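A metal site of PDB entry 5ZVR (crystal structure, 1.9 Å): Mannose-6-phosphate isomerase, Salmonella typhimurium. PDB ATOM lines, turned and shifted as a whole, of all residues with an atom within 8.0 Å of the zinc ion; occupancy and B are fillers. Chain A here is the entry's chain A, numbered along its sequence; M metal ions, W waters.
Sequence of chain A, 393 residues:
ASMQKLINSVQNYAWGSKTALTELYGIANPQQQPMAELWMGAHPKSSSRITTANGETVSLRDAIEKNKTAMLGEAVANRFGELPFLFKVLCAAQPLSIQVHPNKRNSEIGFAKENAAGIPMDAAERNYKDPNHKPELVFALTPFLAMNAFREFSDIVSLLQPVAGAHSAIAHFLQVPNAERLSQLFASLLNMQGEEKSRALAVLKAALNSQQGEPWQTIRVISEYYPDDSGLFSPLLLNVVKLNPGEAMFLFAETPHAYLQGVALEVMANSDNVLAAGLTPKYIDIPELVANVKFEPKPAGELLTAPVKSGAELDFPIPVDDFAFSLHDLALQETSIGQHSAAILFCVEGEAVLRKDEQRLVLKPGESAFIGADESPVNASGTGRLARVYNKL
Water W1 lies within hydrogen-bond range of the side-chain hydroxyl (OH) of Tyr 259 (2.7 Å) and the side-chain carboxylate (OE2) of Glu 136 (3.3 Å).
The zinc ion is bound by water W1 (1.8 Å), NE2 of His 257 (2.1 Å), OE1 of Glu 136 (2.2 Å) and NE2 of His 101 (2.2 Å).
The backbone carbonyl oxygen of His 257 sits at hydrogen-bond distance from the backbone NH of Gln 99 (2.9 Å).
ND1 of His 257 sits at hydrogen-bond distance from O of Thr 255 (3.0 Å).
The side-chain carboxylate (OE1) of Glu 136 sits close to the side-chain hydroxyl (OH) of Tyr 259 (3.3 Å).
N of Leu 251 sits at hydrogen-bond distance from O of Glu 136 (2.7 Å).
The side-chain amino group (NZ) of Lys 134 is in salt-bridge range of the side-chain carboxylate (OE2) of Glu 136 (3.2 Å).
The backbone carbonyl oxygen (O) of Asn 273 is in hydrogen-bond range of a ring nitrogen (ND1) of His 101 (2.7 Å).
The side-chain hydroxyl (OG) of Ser 97 sits at hydrogen-bond distance from the side-chain amide nitrogen (NE2) of Gln 99 (3.5 Å).
Gln 99 touches the zinc ion (OE1 to ZN, 3.4 Å).
Within 4 Å of the zinc ion: Gln 99, His 101, Glu 136 and His 257.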
ATOM      1  N   SER A  97     -21.300  -0.993  21.397  1.00  0.00           N
ATOM      2  CA  SER A  97     -20.954  -0.830  22.789  1.00  0.00           C
ATOM      3  C   SER A  97     -19.565  -0.342  23.049  1.00  0.00           C
ATOM      4  O   SER A  97     -18.643  -0.449  22.215  1.00  0.00           O
ATOM      5  CB  SER A  97     -21.273  -2.142  23.506  1.00  0.00           C
ATOM      6  OG  SER A  97     -20.304  -3.081  23.187  1.00  0.00           O
ATOM      7  N   ILE A  98     -19.366   0.248  24.224  1.00  0.00           N
ATOM      8  CA  ILE A  98     -18.051   0.651  24.612  1.00  0.00           C
ATOM      9  C   ILE A  98     -17.348  -0.611  25.168  1.00  0.00           C
ATOM     10  O   ILE A  98     -17.944  -1.326  26.014  1.00  0.00           O
ATOM     11  CB  ILE A  98     -18.040   1.780  25.699  1.00  0.00           C
ATOM     12  CG1 ILE A  98     -18.957   2.957  25.328  1.00  0.00           C
ATOM     13  CG2 ILE A  98     -16.617   2.294  25.882  1.00  0.00           C
ATOM     14  CD1 ILE A  98     -19.107   4.063  26.367  1.00  0.00           C
ATOM     15  N   GLN A  99     -16.086  -0.841  24.768  1.00  0.00           N
ATOM     16  CA  GLN A  99     -15.442  -2.042  25.163  1.00  0.00           C
ATOM     17  C   GLN A  99     -14.033  -1.769  25.593  1.00  0.00           C
ATOM     18  O   GLN A  99     -13.430  -0.809  25.127  1.00  0.00           O
ATOM     19  CB  GLN A  99     -15.385  -2.970  23.965  1.00  0.00           C
ATOM     20  CG  GLN A  99     -16.734  -3.478  23.499  1.00  0.00           C
ATOM     21  CD  GLN A  99     -16.574  -4.352  22.233  1.00  0.00           C
ATOM     22  OE1 GLN A  99     -15.481  -4.747  21.915  1.00  0.00           O
ATOM     23  NE2 GLN A  99     -17.665  -4.617  21.542  1.00  0.00           N
ATOM     24  N   VAL A 100     -13.526  -2.627  26.458  1.00  0.00           N
ATOM     25  CA  VAL A 100     -12.119  -2.656  26.855  1.00  0.00           C
ATOM     26  C   VAL A 100     -11.575  -4.092  26.750  1.00  0.00           C
ATOM     27  O   VAL A 100     -12.285  -5.004  27.107  1.00  0.00           O
ATOM     28  CB  VAL A 100     -11.958  -2.193  28.328  1.00  0.00           C
ATOM     29  CG1 VAL A 100     -10.567  -2.513  28.963  1.00  0.00           C
ATOM     30  CG2 VAL A 100     -12.392  -0.701  28.438  1.00  0.00           C
ATOM     31  N   HIS A 101     -10.358  -4.253  26.260  1.00  0.00           N
ATOM     32  CA  HIS A 101      -9.705  -5.536  26.234  1.00  0.00           C
ATOM     33  C   HIS A 101      -8.524  -5.529  27.131  1.00  0.00           C
ATOM     34  O   HIS A 101      -7.612  -4.761  26.933  1.00  0.00           O
ATOM     35  CB  HIS A 101      -9.255  -5.917  24.830  1.00  0.00           C
ATOM     36  CG  HIS A 101     -10.359  -5.836  23.868  1.00  0.00           C
ATOM     37  ND1 HIS A 101     -11.512  -6.580  24.019  1.00  0.00           N
ATOM     38  CD2 HIS A 101     -10.580  -4.994  22.841  1.00  0.00           C
ATOM     39  CE1 HIS A 101     -12.373  -6.227  23.084  1.00  0.00           C
ATOM     40  NE2 HIS A 101     -11.821  -5.292  22.340  1.00  0.00           N
ATOM     41  N   LYS A 134      -6.481  -9.001  23.004  1.00  0.00           N
ATOM     42  CA  LYS A 134      -7.216  -8.681  21.786  1.00  0.00           C
ATOM     43  C   LYS A 134      -6.836  -7.330  21.199  1.00  0.00           C
ATOM     44  O   LYS A 134      -7.649  -6.471  21.112  1.00  0.00           O
ATOM     45  CB  LYS A 134      -8.762  -8.758  22.015  1.00  0.00           C
ATOM     46  CG  LYS A 134      -9.544  -9.026  20.778  1.00  0.00           C
ATOM     47  CD  LYS A 134     -10.996  -9.110  21.149  1.00  0.00           C
ATOM     48  CE  LYS A 134     -11.908  -9.639  20.079  1.00  0.00           C
ATOM     49  NZ  LYS A 134     -11.518  -9.342  18.732  1.00  0.00           N
ATOM     50  N   PRO A 135      -5.593  -7.180  20.791  1.00  0.00           N
ATOM     51  CA  PRO A 135      -5.235  -6.089  19.930  1.00  0.00           C
ATOM     52  C   PRO A 135      -6.094  -6.129  18.657  1.00  0.00           C
ATOM     53  O   PRO A 135      -6.486  -7.190  18.181  1.00  0.00           O
ATOM     54  CB  PRO A 135      -3.768  -6.367  19.645  1.00  0.00           C
ATOM     55  CG  PRO A 135      -3.677  -7.831  19.695  1.00  0.00           C
ATOM     56  CD  PRO A 135      -4.525  -8.178  20.887  1.00  0.00           C
ATOM     57  N   GLU A 136      -6.418  -4.946  18.164  1.00  0.00           N
ATOM     58  CA  GLU A 136      -7.207  -4.737  16.979  1.00  0.00           C
ATOM     59  C   GLU A 136      -6.740  -3.476  16.286  1.00  0.00           C
ATOM     60  O   GLU A 136      -6.303  -2.507  16.910  1.00  0.00           O
ATOM     61  CB  GLU A 136      -8.693  -4.529  17.317  1.00  0.00           C
ATOM     62  CG  GLU A 136      -9.318  -5.563  18.228  1.00  0.00           C
ATOM     63  CD  GLU A 136     -10.748  -5.215  18.624  1.00  0.00           C
ATOM     64  OE1 GLU A 136     -10.900  -4.092  19.192  1.00  0.00           O
ATOM     65  OE2 GLU A 136     -11.605  -6.110  18.527  1.00  0.00           O
ATOM     66  N   LEU A 137      -6.974  -3.504  14.989  1.00  0.00           N
ATOM     67  CA  LEU A 137      -6.815  -2.354  14.130  1.00  0.00           C
ATOM     68  C   LEU A 137      -8.033  -2.174  13.305  1.00  0.00           C
ATOM     69  O   LEU A 137      -8.596  -3.162  12.741  1.00  0.00           O
ATOM     70  CB  LEU A 137      -5.603  -2.557  13.221  1.00  0.00           C
ATOM     71  CG  LEU A 137      -5.256  -1.365  12.343  1.00  0.00           C
ATOM     72  CD1 LEU A 137      -4.167  -0.517  12.918  1.00  0.00           C
ATOM     73  CD2 LEU A 137      -4.689  -1.930  11.059  1.00  0.00           C
ATOM     74  N   LEU A 251      -6.321  -0.294  18.451  1.00  0.00           N
ATOM     75  CA  LEU A 251      -6.951  -0.304  19.753  1.00  0.00           C
ATOM     76  C   LEU A 251      -6.098  -1.020  20.769  1.00  0.00           C
ATOM     77  O   LEU A 251      -6.100  -2.240  20.843  1.00  0.00           O
ATOM     78  CB  LEU A 251      -8.317  -0.955  19.663  1.00  0.00           C
ATOM     79  CG  LEU A 251      -9.476  -0.300  18.809  1.00  0.00           C
ATOM     80  CD1 LEU A 251      -9.630   1.182  19.191  1.00  0.00           C
ATOM     81  CD2 LEU A 251      -9.272  -0.433  17.290  1.00  0.00           C
ATOM     82  N   PHE A 252      -5.460  -0.267  21.643  1.00  0.00           N
ATOM     83  CA  PHE A 252      -4.591  -0.775  22.668  1.00  0.00           C
ATOM     84  C   PHE A 252      -5.393  -1.502  23.786  1.00  0.00           C
ATOM     85  O   PHE A 252      -6.609  -1.258  24.030  1.00  0.00           O
ATOM     86  CB  PHE A 252      -3.788   0.422  23.288  1.00  0.00           C
ATOM     87  CG  PHE A 252      -2.708   0.974  22.376  1.00  0.00           C
ATOM     88  CD1 PHE A 252      -1.478   0.399  22.395  1.00  0.00           C
ATOM     89  CD2 PHE A 252      -2.973   2.064  21.509  1.00  0.00           C
ATOM     90  CE1 PHE A 252      -0.452   0.888  21.589  1.00  0.00           C
ATOM     91  CE2 PHE A 252      -1.987   2.532  20.657  1.00  0.00           C
ATOM     92  CZ  PHE A 252      -0.719   1.980  20.713  1.00  0.00           C
ATOM     93  N   THR A 255      -7.963   0.135  27.231  1.00  0.00           N
ATOM     94  CA  THR A 255      -8.331   1.441  26.670  1.00  0.00           C
ATOM     95  C   THR A 255      -9.760   1.393  26.146  1.00  0.00           C
ATOM     96  O   THR A 255     -10.076   0.578  25.259  1.00  0.00           O
ATOM     97  CB  THR A 255      -7.330   1.845  25.556  1.00  0.00           C
ATOM     98  OG1 THR A 255      -5.978   1.813  26.094  1.00  0.00           O
ATOM     99  CG2 THR A 255      -7.653   3.252  25.038  1.00  0.00           C
ATOM    100  N   PRO A 256     -10.645   2.227  26.684  1.00  0.00           N
ATOM    101  CA  PRO A 256     -12.025   2.117  26.208  1.00  0.00           C
ATOM    102  C   PRO A 256     -12.193   2.623  24.777  1.00  0.00           C
ATOM    103  O   PRO A 256     -11.540   3.615  24.410  1.00  0.00           O
ATOM    104  CB  PRO A 256     -12.793   3.047  27.180  1.00  0.00           C
ATOM    105  CG  PRO A 256     -11.932   3.162  28.395  1.00  0.00           C
ATOM    106  CD  PRO A 256     -10.530   3.037  27.928  1.00  0.00           C
ATOM    107  N   HIS A 257     -12.983   1.907  23.973  1.00  0.00           N
ATOM    108  CA  HIS A 257     -13.247   2.375  22.644  1.00  0.00           C
ATOM    109  C   HIS A 257     -14.621   1.942  22.201  1.00  0.00           C
ATOM    110  O   HIS A 257     -15.170   1.051  22.806  1.00  0.00           O
ATOM    111  CB  HIS A 257     -12.156   1.826  21.680  1.00  0.00           C
ATOM    112  CG  HIS A 257     -12.073   0.349  21.687  1.00  0.00           C
ATOM    113  ND1 HIS A 257     -11.400  -0.323  22.675  1.00  0.00           N
ATOM    114  CD2 HIS A 257     -12.597  -0.594  20.879  1.00  0.00           C
ATOM    115  CE1 HIS A 257     -11.569  -1.623  22.511  1.00  0.00           C
ATOM    116  NE2 HIS A 257     -12.271  -1.807  21.419  1.00  0.00           N
ATOM    117  N   ALA A 258     -15.153   2.499  21.099  1.00  0.00           N
ATOM    118  CA  ALA A 258     -16.455   2.112  20.594  1.00  0.00           C
ATOM    119  C   ALA A 258     -16.512   2.437  19.138  1.00  0.00           C
ATOM    120  O   ALA A 258     -16.002   3.488  18.736  1.00  0.00           O
ATOM    121  CB  ALA A 258     -17.568   2.897  21.298  1.00  0.00           C
ATOM    122  N   TYR A 259     -17.210   1.608  18.359  1.00  0.00           N
ATOM    123  CA  TYR A 259     -17.477   1.911  16.963  1.00  0.00           C
ATOM    124  C   TYR A 259     -18.874   2.497  16.832  1.00  0.00           C
ATOM    125  O   TYR A 259     -19.838   1.831  17.193  1.00  0.00           O
ATOM    126  CB  TYR A 259     -17.386   0.624  16.132  1.00  0.00           C
ATOM    127  CG  TYR A 259     -16.057  -0.130  16.361  1.00  0.00           C
ATOM    128  CD1 TYR A 259     -14.877   0.520  16.531  1.00  0.00           C
ATOM    129  CD2 TYR A 259     -16.012  -1.515  16.387  1.00  0.00           C
ATOM    130  CE1 TYR A 259     -13.679  -0.152  16.749  1.00  0.00           C
ATOM    131  CE2 TYR A 259     -14.796  -2.217  16.582  1.00  0.00           C
ATOM    132  CZ  TYR A 259     -13.644  -1.524  16.759  1.00  0.00           C
ATOM    133  OH  TYR A 259     -12.443  -2.179  17.000  1.00  0.00           O
ATOM    134  N   GLU A 266     -11.542  -4.519   9.974  1.00  0.00           N
ATOM    135  CA  GLU A 266     -11.031  -4.703  11.342  1.00  0.00           C
ATOM    136  C   GLU A 266     -10.189  -5.944  11.297  1.00  0.00           C
ATOM    137  O   GLU A 266     -10.596  -6.962  10.749  1.00  0.00           O
ATOM    138  CB  GLU A 266     -12.159  -4.907  12.342  1.00  0.00           C
ATOM    139  CG  GLU A 266     -11.746  -4.932  13.813  1.00  0.00           C
ATOM    140  CD  GLU A 266     -12.946  -5.318  14.677  1.00  0.00           C
ATOM    141  OE1 GLU A 266     -12.989  -4.857  15.844  1.00  0.00           O
ATOM    142  OE2 GLU A 266     -13.822  -6.060  14.153  1.00  0.00           O
ATOM    143  N   MET A 268      -8.206  -8.432  14.094  1.00  0.00           N
ATOM    144  CA  MET A 268      -8.061  -8.677  15.524  1.00  0.00           C
ATOM    145  C   MET A 268      -7.297  -9.966  15.795  1.00  0.00           C
ATOM    146  O   MET A 268      -7.299 -10.893  14.950  1.00  0.00           O
ATOM    147  CB  MET A 268      -9.429  -8.785  16.164  1.00  0.00           C
ATOM    148  CG  MET A 268     -10.162 -10.089  15.840  1.00  0.00           C
ATOM    149  SD  MET A 268     -11.946  -9.886  15.885  1.00  0.00           S
ATOM    150  CE  MET A 268     -11.965  -8.593  14.650  1.00  0.00           C
ATOM    151  N   ASN A 273     -12.370 -11.826  25.059  1.00  0.00           N
ATOM    152  CA  ASN A 273     -12.391 -11.099  26.320  1.00  0.00           C
ATOM    153  C   ASN A 273     -12.837  -9.683  25.962  1.00  0.00           C
ATOM    154  O   ASN A 273     -12.047  -8.910  25.353  1.00  0.00           O
ATOM    155  CB  ASN A 273     -11.020 -11.124  26.970  1.00  0.00           C
ATOM    156  CG  ASN A 273     -10.529 -12.521  27.194  1.00  0.00           C
ATOM    157  OD1 ASN A 273     -11.329 -13.464  27.188  1.00  0.00           O
ATOM    158  ND2 ASN A 273      -9.223 -12.676  27.421  1.00  0.00           N
ATOM    159  N   VAL A 274     -14.101  -9.379  26.263  1.00  0.00           N
ATOM    160  CA  VAL A 274     -14.588  -8.014  26.095  1.00  0.00           C
ATOM    161  C   VAL A 274     -15.126  -7.591  27.404  1.00  0.00           C
ATOM    162  O   VAL A 274     -15.864  -8.312  28.032  1.00  0.00           O
ATOM    163  CB  VAL A 274     -15.626  -7.881  24.948  1.00  0.00           C
ATOM    164  CG1 VAL A 274     -15.977  -6.395  24.665  1.00  0.00           C
ATOM    165  CG2 VAL A 274     -15.101  -8.559  23.692  1.00  0.00           C
ATOM    166  N   LEU A 275     -14.611  -6.506  27.927  1.00  0.00           N
ATOM    167  CA  LEU A 275     -15.178  -5.954  29.114  1.00  0.00           C
ATOM    168  C   LEU A 275     -16.003  -4.779  28.676  1.00  0.00           C
ATOM    169  O   LEU A 275     -15.464  -3.852  28.092  1.00  0.00           O
ATOM    170  CB  LEU A 275     -14.064  -5.543  30.053  1.00  0.00           C
ATOM    171  CG  LEU A 275     -13.255  -6.628  30.683  1.00  0.00           C
ATOM    172  CD1 LEU A 275     -12.081  -5.981  31.436  1.00  0.00           C
ATOM    173  CD2 LEU A 275     -14.099  -7.559  31.578  1.00  0.00           C
HETATM  174 ZN    ZN M   1     -12.422  -3.830  20.755  1.00  0.00          ZN
HETATM  175  O   HOH W   1     -13.325  -3.352  19.236  1.00  0.00           O
